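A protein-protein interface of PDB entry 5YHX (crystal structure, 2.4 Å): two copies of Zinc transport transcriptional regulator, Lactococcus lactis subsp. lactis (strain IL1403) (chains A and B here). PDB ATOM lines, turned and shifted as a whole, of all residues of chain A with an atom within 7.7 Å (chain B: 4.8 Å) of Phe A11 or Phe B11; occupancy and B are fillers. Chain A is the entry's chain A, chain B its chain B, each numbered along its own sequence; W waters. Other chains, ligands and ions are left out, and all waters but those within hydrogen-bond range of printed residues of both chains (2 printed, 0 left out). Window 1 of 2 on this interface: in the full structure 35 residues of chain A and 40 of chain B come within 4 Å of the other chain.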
ATOM      1  N   LEU A   4     -27.559 -19.263 -35.120  1.00  0.00           N
ATOM      2  CA  LEU A   4     -27.042 -20.443 -34.450  1.00  0.00           C
ATOM      3  C   LEU A   4     -26.373 -20.032 -33.144  1.00  0.00           C
ATOM      4  O   LEU A   4     -26.537 -20.690 -32.118  1.00  0.00           O
ATOM      5  CB  LEU A   4     -26.038 -21.178 -35.338  1.00  0.00           C
ATOM      6  CG  LEU A   4     -25.619 -22.584 -34.884  1.00  0.00           C
ATOM      7  CD1 LEU A   4     -26.762 -23.589 -35.025  1.00  0.00           C
ATOM      8  CD2 LEU A   4     -24.403 -23.076 -35.654  1.00  0.00           C
ATOM      9  N   ALA A   5     -25.622 -18.940 -33.185  1.00  0.00           N
ATOM     10  CA  ALA A   5     -24.879 -18.527 -32.009  1.00  0.00           C
ATOM     11  C   ALA A   5     -25.842 -18.292 -30.854  1.00  0.00           C
ATOM     12  O   ALA A   5     -25.513 -18.568 -29.695  1.00  0.00           O
ATOM     13  CB  ALA A   5     -24.070 -17.285 -32.292  1.00  0.00           C
ATOM     14  N   ASN A   6     -27.031 -17.790 -31.179  1.00  0.00           N
ATOM     15  CA  ASN A   6     -28.039 -17.500 -30.165  1.00  0.00           C
ATOM     16  C   ASN A   6     -28.614 -18.768 -29.548  1.00  0.00           C
ATOM     17  O   ASN A   6     -28.777 -18.853 -28.338  1.00  0.00           O
ATOM     18  CB  ASN A   6     -29.152 -16.597 -30.717  1.00  0.00           C
ATOM     19  CG  ASN A   6     -28.866 -15.111 -30.494  1.00  0.00           C
ATOM     20  OD1 ASN A   6     -28.258 -14.728 -29.492  1.00  0.00           O
ATOM     21  ND2 ASN A   6     -29.300 -14.272 -31.429  1.00  0.00           N
ATOM     22  N   GLN A   7     -28.898 -19.760 -30.383  1.00  0.00           N
ATOM     23  CA  GLN A   7     -29.384 -21.039 -29.893  1.00  0.00           C
ATOM     24  C   GLN A   7     -28.318 -21.732 -29.030  1.00  0.00           C
ATOM     25  O   GLN A   7     -28.616 -22.253 -27.947  1.00  0.00           O
ATOM     26  CB  GLN A   7     -29.794 -21.932 -31.054  1.00  0.00           C
ATOM     27  CG  GLN A   7     -30.653 -23.114 -30.635  1.00  0.00           C
ATOM     28  CD  GLN A   7     -31.008 -24.035 -31.797  1.00  0.00           C
ATOM     29  OE1 GLN A   7     -30.435 -23.932 -32.888  1.00  0.00           O
ATOM     30  NE2 GLN A   7     -31.959 -24.944 -31.564  1.00  0.00           N
ATOM     31  N   ILE A   8     -27.078 -21.726 -29.501  1.00  0.00           N
ATOM     32  CA  ILE A   8     -25.981 -22.254 -28.699  1.00  0.00           C
ATOM     33  C   ILE A   8     -25.942 -21.575 -27.330  1.00  0.00           C
ATOM     34  O   ILE A   8     -25.771 -22.235 -26.323  1.00  0.00           O
ATOM     35  CB  ILE A   8     -24.602 -22.078 -29.381  1.00  0.00           C
ATOM     36  CG1 ILE A   8     -24.541 -22.835 -30.694  1.00  0.00           C
ATOM     37  CG2 ILE A   8     -23.503 -22.589 -28.495  1.00  0.00           C
ATOM     38  CD1 ILE A   8     -23.200 -22.725 -31.362  1.00  0.00           C
ATOM     39  N   ASP A   9     -26.088 -20.257 -27.308  1.00  0.00           N
ATOM     40  CA  ASP A   9     -25.994 -19.487 -26.075  1.00  0.00           C
ATOM     41  C   ASP A   9     -27.097 -19.889 -25.122  1.00  0.00           C
ATOM     42  O   ASP A   9     -26.833 -20.179 -23.968  1.00  0.00           O
ATOM     43  CB  ASP A   9     -26.095 -17.994 -26.372  1.00  0.00           C
ATOM     44  CG  ASP A   9     -25.623 -17.121 -25.207  1.00  0.00           C
ATOM     45  OD1 ASP A   9     -24.517 -17.391 -24.670  1.00  0.00           O
ATOM     46  OD2 ASP A   9     -26.356 -16.162 -24.833  1.00  0.00           O
ATOM     47  N   GLN A  10     -28.330 -19.900 -25.628  1.00  0.00           N
ATOM     48  CA  GLN A  10     -29.521 -20.292 -24.876  1.00  0.00           C
ATOM     49  C   GLN A  10     -29.443 -21.744 -24.427  1.00  0.00           C
ATOM     50  O   GLN A  10     -29.901 -22.099 -23.339  1.00  0.00           O
ATOM     51  CB  GLN A  10     -30.798 -20.137 -25.727  1.00  0.00           C
ATOM     52  CG  GLN A  10     -31.165 -18.706 -26.177  1.00  0.00           C
ATOM     53  CD  GLN A  10     -30.979 -17.661 -25.069  1.00  0.00           C
ATOM     54  OE1 GLN A  10     -31.614 -17.728 -23.998  1.00  0.00           O
ATOM     55  NE2 GLN A  10     -30.093 -16.689 -25.324  1.00  0.00           N
ATOM     56  N   PHE A  11     -28.899 -22.598 -25.286  1.00  0.00           N
ATOM     57  CA  PHE A  11     -28.838 -24.002 -24.976  1.00  0.00           C
ATOM     58  C   PHE A  11     -27.931 -24.207 -23.790  1.00  0.00           C
ATOM     59  O   PHE A  11     -28.194 -25.051 -22.941  1.00  0.00           O
ATOM     60  CB  PHE A  11     -28.307 -24.798 -26.153  1.00  0.00           C
ATOM     61  CG  PHE A  11     -27.825 -26.164 -25.780  1.00  0.00           C
ATOM     62  CD1 PHE A  11     -28.724 -27.183 -25.544  1.00  0.00           C
ATOM     63  CD2 PHE A  11     -26.469 -26.425 -25.656  1.00  0.00           C
ATOM     64  CE1 PHE A  11     -28.286 -28.438 -25.211  1.00  0.00           C
ATOM     65  CE2 PHE A  11     -26.025 -27.685 -25.327  1.00  0.00           C
ATOM     66  CZ  PHE A  11     -26.936 -28.695 -25.106  1.00  0.00           C
ATOM     67  N   LEU A  12     -26.858 -23.438 -23.731  1.00  0.00           N
ATOM     68  CA  LEU A  12     -25.935 -23.563 -22.623  1.00  0.00           C
ATOM     69  C   LEU A  12     -26.601 -23.049 -21.341  1.00  0.00           C
ATOM     70  O   LEU A  12     -26.451 -23.638 -20.280  1.00  0.00           O
ATOM     71  CB  LEU A  12     -24.630 -22.819 -22.921  1.00  0.00           C
ATOM     72  CG  LEU A  12     -23.788 -23.376 -24.078  1.00  0.00           C
ATOM     73  CD1 LEU A  12     -22.549 -22.537 -24.325  1.00  0.00           C
ATOM     74  CD2 LEU A  12     -23.376 -24.799 -23.815  1.00  0.00           C
ATOM     75  N   GLY A  13     -27.347 -21.956 -21.446  1.00  0.00           N
ATOM     76  CA  GLY A  13     -28.047 -21.422 -20.298  1.00  0.00           C
ATOM     77  C   GLY A  13     -28.997 -22.475 -19.758  1.00  0.00           C
ATOM     78  O   GLY A  13     -29.058 -22.721 -18.553  1.00  0.00           O
ATOM     79  N   THR A  14     -29.727 -23.112 -20.668  1.00  0.00           N
ATOM     80  CA  THR A  14     -30.614 -24.219 -20.326  1.00  0.00           C
ATOM     81  C   THR A  14     -29.883 -25.341 -19.615  1.00  0.00           C
ATOM     82  O   THR A  14     -30.407 -25.925 -18.683  1.00  0.00           O
ATOM     83  CB  THR A  14     -31.294 -24.784 -21.575  1.00  0.00           C
ATOM     84  OG1 THR A  14     -32.245 -23.834 -22.055  1.00  0.00           O
ATOM     85  CG2 THR A  14     -32.003 -26.070 -21.267  1.00  0.00           C
ATOM     86  N   ILE A  15     -28.658 -25.629 -20.033  1.00  0.00           N
ATOM     87  CA  ILE A  15     -27.886 -26.680 -19.383  1.00  0.00           C
ATOM     88  C   ILE A  15     -27.619 -26.328 -17.926  1.00  0.00           C
ATOM     89  O   ILE A  15     -27.558 -27.194 -17.059  1.00  0.00           O
ATOM     90  CB  ILE A  15     -26.558 -26.980 -20.101  1.00  0.00           C
ATOM     91  CG1 ILE A  15     -26.817 -27.643 -21.450  1.00  0.00           C
ATOM     92  CG2 ILE A  15     -25.738 -27.906 -19.285  1.00  0.00           C
ATOM     93  CD1 ILE A  15     -27.800 -28.794 -21.361  1.00  0.00           C
ATOM     94  N   MET A  16     -27.462 -25.051 -17.640  1.00  0.00           N
ATOM     95  CA  MET A  16     -27.226 -24.669 -16.268  1.00  0.00           C
ATOM     96  C   MET A  16     -28.477 -24.570 -15.386  1.00  0.00           C
ATOM     97  O   MET A  16     -28.456 -25.015 -14.239  1.00  0.00           O
ATOM     98  CB  MET A  16     -26.392 -23.417 -16.238  1.00  0.00           C
ATOM     99  CG  MET A  16     -25.005 -23.706 -16.752  1.00  0.00           C
ATOM    100  SD  MET A  16     -24.188 -22.152 -16.831  1.00  0.00           S
ATOM    101  CE  MET A  16     -24.360 -21.654 -15.121  1.00  0.00           C
ATOM    102  N   GLN A  17     -29.567 -24.020 -15.906  1.00  0.00           N
ATOM    103  CA  GLN A  17     -30.816 -24.045 -15.139  1.00  0.00           C
ATOM    104  C   GLN A  17     -31.196 -25.476 -14.782  1.00  0.00           C
ATOM    105  O   GLN A  17     -31.805 -25.725 -13.740  1.00  0.00           O
ATOM    106  CB  GLN A  17     -31.960 -23.353 -15.881  1.00  0.00           C
ATOM    107  CG  GLN A  17     -31.832 -21.841 -15.870  1.00  0.00           C
ATOM    108  CD  GLN A  17     -32.248 -21.223 -17.183  1.00  0.00           C
ATOM    109  OE1 GLN A  17     -32.910 -21.867 -18.007  1.00  0.00           O
ATOM    110  NE2 GLN A  17     -31.855 -19.966 -17.395  1.00  0.00           N
ATOM    111  N   ILE A  25     -25.102 -34.253 -14.648  1.00  0.00           N
ATOM    112  CA  ILE A  25     -26.330 -34.346 -15.422  1.00  0.00           C
ATOM    113  C   ILE A  25     -26.802 -35.795 -15.558  1.00  0.00           C
ATOM    114  O   ILE A  25     -26.153 -36.606 -16.214  1.00  0.00           O
ATOM    115  CB  ILE A  25     -26.125 -33.774 -16.825  1.00  0.00           C
ATOM    116  CG1 ILE A  25     -25.576 -32.356 -16.749  1.00  0.00           C
ATOM    117  CG2 ILE A  25     -27.431 -33.745 -17.593  1.00  0.00           C
ATOM    118  CD1 ILE A  25     -26.583 -31.361 -16.225  1.00  0.00           C
ATOM    119  N   PHE A 137     -19.484 -30.718 -34.536  1.00  0.00           N
ATOM    120  CA  PHE A 137     -19.951 -29.533 -33.808  1.00  0.00           C
ATOM    121  C   PHE A 137     -19.531 -29.597 -32.333  1.00  0.00           C
ATOM    122  O   PHE A 137     -18.930 -28.661 -31.804  1.00  0.00           O
ATOM    123  CB  PHE A 137     -21.462 -29.385 -33.918  1.00  0.00           C
ATOM    124  CG  PHE A 137     -22.038 -28.370 -32.970  1.00  0.00           C
ATOM    125  CD1 PHE A 137     -21.751 -27.020 -33.119  1.00  0.00           C
ATOM    126  CD2 PHE A 137     -22.871 -28.766 -31.930  1.00  0.00           C
ATOM    127  CE1 PHE A 137     -22.272 -26.091 -32.257  1.00  0.00           C
ATOM    128  CE2 PHE A 137     -23.402 -27.829 -31.062  1.00  0.00           C
ATOM    129  CZ  PHE A 137     -23.101 -26.487 -31.228  1.00  0.00           C
ATOM    130  N   LEU A 138     -19.807 -30.731 -31.695  1.00  0.00           N
ATOM    131  CA  LEU A 138     -19.467 -30.927 -30.286  1.00  0.00           C
ATOM    132  C   LEU A 138     -17.961 -30.875 -29.996  1.00  0.00           C
ATOM    133  O   LEU A 138     -17.561 -30.390 -28.930  1.00  0.00           O
ATOM    134  CB  LEU A 138     -20.088 -32.227 -29.739  1.00  0.00           C
ATOM    135  CG  LEU A 138     -21.624 -32.225 -29.619  1.00  0.00           C
ATOM    136  CD1 LEU A 138     -22.158 -33.612 -29.364  1.00  0.00           C
ATOM    137  CD2 LEU A 138     -22.063 -31.318 -28.502  1.00  0.00           C
ATOM    138  N   SER A 139     -17.136 -31.371 -30.924  1.00  0.00           N
ATOM    139  CA  SER A 139     -15.678 -31.317 -30.744  1.00  0.00           C
ATOM    140  C   SER A 139     -15.234 -29.874 -30.798  1.00  0.00           C
ATOM    141  O   SER A 139     -14.436 -29.433 -29.987  1.00  0.00           O
ATOM    142  CB  SER A 139     -14.924 -32.108 -31.829  1.00  0.00           C
ATOM    143  OG  SER A 139     -15.261 -33.484 -31.819  1.00  0.00           O
ATOM    144  N   ALA A 140     -15.774 -29.155 -31.769  1.00  0.00           N
ATOM    145  CA  ALA A 140     -15.451 -27.755 -31.978  1.00  0.00           C
ATOM    146  C   ALA A 140     -15.839 -26.979 -30.728  1.00  0.00           C
ATOM    147  O   ALA A 140     -14.990 -26.358 -30.081  1.00  0.00           O
ATOM    148  CB  ALA A 140     -16.208 -27.233 -33.168  1.00  0.00           C
ATOM    149  N   LEU A 141     -17.128 -27.038 -30.385  1.00  0.00           N
ATOM    150  CA  LEU A 141     -17.644 -26.378 -29.184  1.00  0.00           C
ATOM    151  C   LEU A 141     -16.880 -26.815 -27.923  1.00  0.00           C
ATOM    152  O   LEU A 141     -16.597 -25.985 -27.076  1.00  0.00           O
ATOM    153  CB  LEU A 141     -19.167 -26.594 -29.037  1.00  0.00           C
ATOM    154  CG  LEU A 141     -19.969 -25.748 -28.033  1.00  0.00           C
ATOM    155  CD1 LEU A 141     -19.874 -24.267 -28.371  1.00  0.00           C
ATOM    156  CD2 LEU A 141     -21.423 -26.167 -28.014  1.00  0.00           C
ATOM    157  N   THR A 142     -16.528 -28.097 -27.799  1.00  0.00           N
ATOM    158  CA  THR A 142     -15.774 -28.556 -26.616  1.00  0.00           C
ATOM    159  C   THR A 142     -14.425 -27.831 -26.433  1.00  0.00           C
ATOM    160  O   THR A 142     -13.887 -27.760 -25.326  1.00  0.00           O
ATOM    161  CB  THR A 142     -15.528 -30.095 -26.614  1.00  0.00           C
ATOM    162  OG1 THR A 142     -16.735 -30.788 -26.265  1.00  0.00           O
ATOM    163  CG2 THR A 142     -14.469 -30.474 -25.593  1.00  0.00           C
ATOM    164  N   GLU A 143     -13.877 -27.281 -27.508  1.00  0.00           N
ATOM    165  CA  GLU A 143     -12.580 -26.623 -27.397  1.00  0.00           C
ATOM    166  C   GLU A 143     -12.630 -25.247 -26.715  1.00  0.00           C
ATOM    167  O   GLU A 143     -11.737 -24.895 -25.954  1.00  0.00           O
ATOM    168  CB  GLU A 143     -11.896 -26.544 -28.758  1.00  0.00           C
ATOM    169  CG  GLU A 143     -11.262 -27.853 -29.171  1.00  0.00           C
ATOM    170  CD  GLU A 143     -10.228 -27.662 -30.262  1.00  0.00           C
ATOM    171  OE1 GLU A 143     -10.359 -26.694 -31.050  1.00  0.00           O
ATOM    172  OE2 GLU A 143      -9.276 -28.476 -30.322  1.00  0.00           O
ATOM    173  N   PHE A 145     -14.258 -24.336 -24.246  1.00  0.00           N
ATOM    174  CA  PHE A 145     -14.281 -24.483 -22.787  1.00  0.00           C
ATOM    175  C   PHE A 145     -13.065 -25.205 -22.199  1.00  0.00           C
ATOM    176  O   PHE A 145     -13.146 -25.803 -21.113  1.00  0.00           O
ATOM    177  CB  PHE A 145     -15.579 -25.146 -22.344  1.00  0.00           C
ATOM    178  CG  PHE A 145     -16.787 -24.505 -22.939  1.00  0.00           C
ATOM    179  CD1 PHE A 145     -17.197 -23.250 -22.508  1.00  0.00           C
ATOM    180  CD2 PHE A 145     -17.488 -25.132 -23.957  1.00  0.00           C
ATOM    181  CE1 PHE A 145     -18.296 -22.631 -23.070  1.00  0.00           C
ATOM    182  CE2 PHE A 145     -18.590 -24.533 -24.522  1.00  0.00           C
ATOM    183  CZ  PHE A 145     -18.997 -23.269 -24.078  1.00  0.00           C
ATOM    184  N   GLN B   7     -20.098 -38.956 -26.342  1.00  0.00           N
ATOM    185  CA  GLN B   7     -19.578 -37.629 -26.628  1.00  0.00           C
ATOM    186  C   GLN B   7     -20.472 -36.536 -26.043  1.00  0.00           C
ATOM    187  O   GLN B   7     -19.971 -35.535 -25.543  1.00  0.00           O
ATOM    188  CB  GLN B   7     -19.357 -37.424 -28.129  1.00  0.00           C
ATOM    189  CG  GLN B   7     -18.550 -36.200 -28.472  1.00  0.00           C
ATOM    190  CD  GLN B   7     -18.335 -36.028 -29.977  1.00  0.00           C
ATOM    191  OE1 GLN B   7     -18.664 -36.907 -30.769  1.00  0.00           O
ATOM    192  NE2 GLN B   7     -17.788 -34.884 -30.368  1.00  0.00           N
ATOM    193  N   ILE B   8     -21.792 -36.708 -26.141  1.00  0.00           N
ATOM    194  CA  ILE B   8     -22.746 -35.747 -25.565  1.00  0.00           C
ATOM    195  C   ILE B   8     -22.529 -35.684 -24.050  1.00  0.00           C
ATOM    196  O   ILE B   8     -22.419 -34.630 -23.455  1.00  0.00           O
ATOM    197  CB  ILE B   8     -24.194 -36.173 -25.870  1.00  0.00           C
ATOM    198  CG1 ILE B   8     -24.536 -35.892 -27.321  1.00  0.00           C
ATOM    199  CG2 ILE B   8     -25.209 -35.481 -24.944  1.00  0.00           C
ATOM    200  CD1 ILE B   8     -25.651 -36.756 -27.849  1.00  0.00           C
ATOM    201  N   ASP B   9     -22.442 -36.852 -23.447  1.00  0.00           N
ATOM    202  CA  ASP B   9     -22.174 -36.987 -22.022  1.00  0.00           C
ATOM    203  C   ASP B   9     -20.923 -36.225 -21.555  1.00  0.00           C
ATOM    204  O   ASP B   9     -20.995 -35.390 -20.670  1.00  0.00           O
ATOM    205  CB  ASP B   9     -22.059 -38.470 -21.665  1.00  0.00           C
ATOM    206  CG  ASP B   9     -22.255 -38.726 -20.185  1.00  0.00           C
ATOM    207  OD1 ASP B   9     -23.409 -38.571 -19.697  1.00  0.00           O
ATOM    208  OD2 ASP B   9     -21.254 -39.078 -19.515  1.00  0.00           O
ATOM    209  N   GLN B  10     -19.774 -36.529 -22.141  1.00  0.00           N
ATOM    210  CA  GLN B  10     -18.545 -35.806 -21.834  1.00  0.00           C
ATOM    211  C   GLN B  10     -18.727 -34.309 -22.025  1.00  0.00           C
ATOM    212  O   GLN B  10     -18.219 -33.492 -21.261  1.00  0.00           O
ATOM    213  CB  GLN B  10     -17.433 -36.266 -22.764  1.00  0.00           C
ATOM    214  CG  GLN B  10     -16.962 -37.676 -22.497  1.00  0.00           C
ATOM    215  CD  GLN B  10     -15.565 -37.679 -21.931  1.00  0.00           C
ATOM    216  OE1 GLN B  10     -14.580 -37.597 -22.681  1.00  0.00           O
ATOM    217  NE2 GLN B  10     -15.463 -37.738 -20.596  1.00  0.00           N
ATOM    218  N   PHE B  11     -19.454 -33.951 -23.064  1.00  0.00           N
ATOM    219  CA  PHE B  11     -19.611 -32.558 -23.362  1.00  0.00           C
ATOM    220  C   PHE B  11     -20.388 -31.860 -22.259  1.00  0.00           C
ATOM    221  O   PHE B  11     -19.963 -30.816 -21.769  1.00  0.00           O
ATOM    222  CB  PHE B  11     -20.301 -32.376 -24.696  1.00  0.00           C
ATOM    223  CG  PHE B  11     -20.790 -31.007 -24.896  1.00  0.00           C
ATOM    224  CD1 PHE B  11     -19.889 -29.968 -25.028  1.00  0.00           C
ATOM    225  CD2 PHE B  11     -22.140 -30.742 -24.920  1.00  0.00           C
ATOM    226  CE1 PHE B  11     -20.327 -28.683 -25.201  1.00  0.00           C
ATOM    227  CE2 PHE B  11     -22.592 -29.458 -25.093  1.00  0.00           C
ATOM    228  CZ  PHE B  11     -21.681 -28.421 -25.231  1.00  0.00           C
ATOM    229  N   LEU B  12     -21.526 -32.425 -21.852  1.00  0.00           N
ATOM    230  CA  LEU B  12     -22.269 -31.797 -20.755  1.00  0.00           C
ATOM    231  C   LEU B  12     -21.395 -31.730 -19.500  1.00  0.00           C
ATOM    232  O   LEU B  12     -21.454 -30.764 -18.743  1.00  0.00           O
ATOM    233  CB  LEU B  12     -23.603 -32.498 -20.502  1.00  0.00           C
ATOM    234  CG  LEU B  12     -24.557 -32.440 -21.706  1.00  0.00           C
ATOM    235  CD1 LEU B  12     -25.526 -33.605 -21.713  1.00  0.00           C
ATOM    236  CD2 LEU B  12     -25.288 -31.152 -21.719  1.00  0.00           C
ATOM    237  N   GLY B  13     -20.551 -32.738 -19.312  1.00  0.00           N
ATOM    238  CA  GLY B  13     -19.609 -32.737 -18.206  1.00  0.00           C
ATOM    239  C   GLY B  13     -18.647 -31.557 -18.290  1.00  0.00           C
ATOM    240  O   GLY B  13     -18.259 -30.970 -17.286  1.00  0.00           O
ATOM    241  N   THR B  14     -18.270 -31.199 -19.506  1.00  0.00           N
ATOM    242  CA  THR B  14     -17.325 -30.119 -19.721  1.00  0.00           C
ATOM    243  C   THR B  14     -17.968 -28.782 -19.401  1.00  0.00           C
ATOM    244  O   THR B  14     -17.411 -28.023 -18.630  1.00  0.00           O
ATOM    245  CB  THR B  14     -16.753 -30.157 -21.145  1.00  0.00           C
ATOM    246  OG1 THR B  14     -15.814 -31.233 -21.218  1.00  0.00           O
ATOM    247  CG2 THR B  14     -16.056 -28.849 -21.487  1.00  0.00           C
ATOM    248  N   ILE B  15     -19.139 -28.507 -19.970  1.00  0.00           N
ATOM    249  CA  ILE B  15     -19.970 -27.394 -19.521  1.00  0.00           C
ATOM    250  C   ILE B  15     -20.058 -27.339 -17.990  1.00  0.00           C
ATOM    251  O   ILE B  15     -19.892 -26.289 -17.419  1.00  0.00           O
ATOM    252  CB  ILE B  15     -21.412 -27.504 -20.032  1.00  0.00           C
ATOM    253  CG1 ILE B  15     -21.441 -27.638 -21.553  1.00  0.00           C
ATOM    254  CG2 ILE B  15     -22.210 -26.293 -19.606  1.00  0.00           C
ATOM    255  CD1 ILE B  15     -20.647 -26.572 -22.257  1.00  0.00           C
ATOM    256  N   LEU B 138     -29.743 -29.549 -31.412  1.00  0.00           N
ATOM    257  CA  LEU B 138     -29.792 -28.757 -30.200  1.00  0.00           C
ATOM    258  C   LEU B 138     -31.204 -28.740 -29.609  1.00  0.00           C
ATOM    259  O   LEU B 138     -31.367 -28.955 -28.409  1.00  0.00           O
ATOM    260  CB  LEU B 138     -29.321 -27.323 -30.449  1.00  0.00           C
ATOM    261  CG  LEU B 138     -27.856 -27.063 -30.792  1.00  0.00           C
ATOM    262  CD1 LEU B 138     -27.707 -25.588 -31.077  1.00  0.00           C
ATOM    263  CD2 LEU B 138     -26.911 -27.481 -29.659  1.00  0.00           C
ATOM    264  N   LEU B 141     -32.032 -31.888 -27.985  1.00  0.00           N
ATOM    265  CA  LEU B 141     -31.316 -32.065 -26.717  1.00  0.00           C
ATOM    266  C   LEU B 141     -31.918 -31.176 -25.624  1.00  0.00           C
ATOM    267  O   LEU B 141     -32.075 -31.597 -24.470  1.00  0.00           O
ATOM    268  CB  LEU B 141     -29.824 -31.766 -26.886  1.00  0.00           C
ATOM    269  CG  LEU B 141     -28.890 -32.196 -25.743  1.00  0.00           C
ATOM    270  CD1 LEU B 141     -29.243 -33.575 -25.224  1.00  0.00           C
ATOM    271  CD2 LEU B 141     -27.430 -32.168 -26.193  1.00  0.00           C
ATOM    272  N   THR B 142     -32.235 -29.941 -26.000  1.00  0.00           N
ATOM    273  CA  THR B 142     -32.953 -29.032 -25.132  1.00  0.00           C
ATOM    274  C   THR B 142     -34.241 -29.684 -24.615  1.00  0.00           C
ATOM    275  O   THR B 142     -34.544 -29.604 -23.431  1.00  0.00           O
ATOM    276  CB  THR B 142     -33.316 -27.734 -25.863  1.00  0.00           C
ATOM    277  OG1 THR B 142     -32.120 -26.989 -26.121  1.00  0.00           O
ATOM    278  CG2 THR B 142     -34.258 -26.896 -25.005  1.00  0.00           C
ATOM    279  N   PHE B 145     -34.015 -31.606 -21.426  1.00  0.00           N
ATOM    280  CA  PHE B 145     -33.785 -30.921 -20.136  1.00  0.00           C
ATOM    281  C   PHE B 145     -34.890 -29.915 -19.769  1.00  0.00           C
ATOM    282  O   PHE B 145     -34.586 -28.789 -19.337  1.00  0.00           O
ATOM    283  CB  PHE B 145     -32.420 -30.181 -20.099  1.00  0.00           C
ATOM    284  CG  PHE B 145     -31.235 -31.044 -20.441  1.00  0.00           C
ATOM    285  CD1 PHE B 145     -30.752 -31.972 -19.534  1.00  0.00           C
ATOM    286  CD2 PHE B 145     -30.602 -30.922 -21.668  1.00  0.00           C
ATOM    287  CE1 PHE B 145     -29.672 -32.775 -19.846  1.00  0.00           C
ATOM    288  CE2 PHE B 145     -29.517 -31.715 -21.989  1.00  0.00           C
ATOM    289  CZ  PHE B 145     -29.052 -32.648 -21.081  1.00  0.00           C
HETATM  290  O   HOH W   1     -25.317 -36.542 -18.821  1.00  0.00           O
HETATM  291  O   HOH W   2     -16.663 -33.383 -28.021  1.00  0.00           O
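Of the printed residues of chain B, Phe A11 touches Phe B11, Leu B141 and Thr B142. Of the printed residues of chain B, Ile A25 touches Phe B145. Phe B11 touches just these residues of chain A: Phe A11 (3.9 Å), Leu A138 (3.6 Å), Leu A141 (3.6 Å) and Thr A142 (3.5 Å). Printed residues of chain A within 4 Å of Leu B12: Ile A15.
O of Gln B10 lies within hydrogen-bond range of OG1 of Thr B14 (3.3 Å). The backbone carbonyl oxygen (O) of Leu B138 sits at hydrogen-bond distance from the side-chain hydroxyl (OG1) of Thr B142, 3.1 Å away. The backbone carbonyl oxygen (O) of Leu A138 sits at hydrogen-bond distance from the side-chain hydroxyl (OG1) of Thr A142 (2.8 Å).
The side-chain amide nitrogen (NE2) of Gln B7 sits at hydrogen-bond distance from the side-chain hydroxyl (OG) of Ser A139, 3.2 Å away.
Gln A7 touches Leu B138, and with the chains exchanged Leu A138 touches Gln B7. Phe A11 touches Thr B142, and with the chains exchanged Thr A142 touches Phe B11. Leu A12 touches Ile B15, and with the chains exchanged Ile A15 touches Leu B12. Ile A15 touches its own counterpart, Ile B15. Positions printed for both chains: 7, 8, 9, 10, 11, 12, 13, 14, 15, 138, 141, 142 and 145. Of the 18 pairs that touch across the chains among the printed residues, 12 have their exchanged pair printed and touching as well.
Water W1 bridges the backbone carbonyl oxygen of Ile A25 (2.7 Å) and the side-chain carboxylate of Asp B9 (2.9 Å). Water W2 lies within hydrogen-bond range of NE2 of Gln B7 (3.0 Å), OG1 of Thr A142 (3.1 Å) and O of Leu A138 (3.3 Å).
OE1 of Gln A7 touches CD1 of Leu B138, 3.7 Å away. CE2 of Phe A11 touches CE2 of Phe B11, at 3.9 Å. Leu B141 touches Phe A11 (CD2 to CZ, 3.7 Å). Phe A11 touches Thr B142 (CD1 to OG1, 3.5 Å). Leu A12 touches Ile B15. Ile A15 touches Phe B145 (CD1 to CE2, 3.4 Å). Gln B7 touches Leu A138 (NE2 to CB, 3.6 Å). Ile B8 touches Leu A138. CD2 of Phe B11 touches CD2 of Leu A138 (3.6 Å). CE2 of Phe A145 touches CD1 of Ile B15, 3.7 Å away.
Hydrophobic or aromatic side chains of chain B within 4 Å of the printed part of chain A: Ile B8, Phe B11, Leu B12, Ile B15, Leu B138, Leu B141 and Phe B145. Of the 23 printed residues of chain A, 11 touch a printed residue of chain B. Hydrophobic or aromatic side chains of chain A within 4 Å of the printed part of chain B: Phe A11, Leu A12, Ile A15, Ile A25, Phe A137, Leu A138, Leu A141 and Phe A145.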
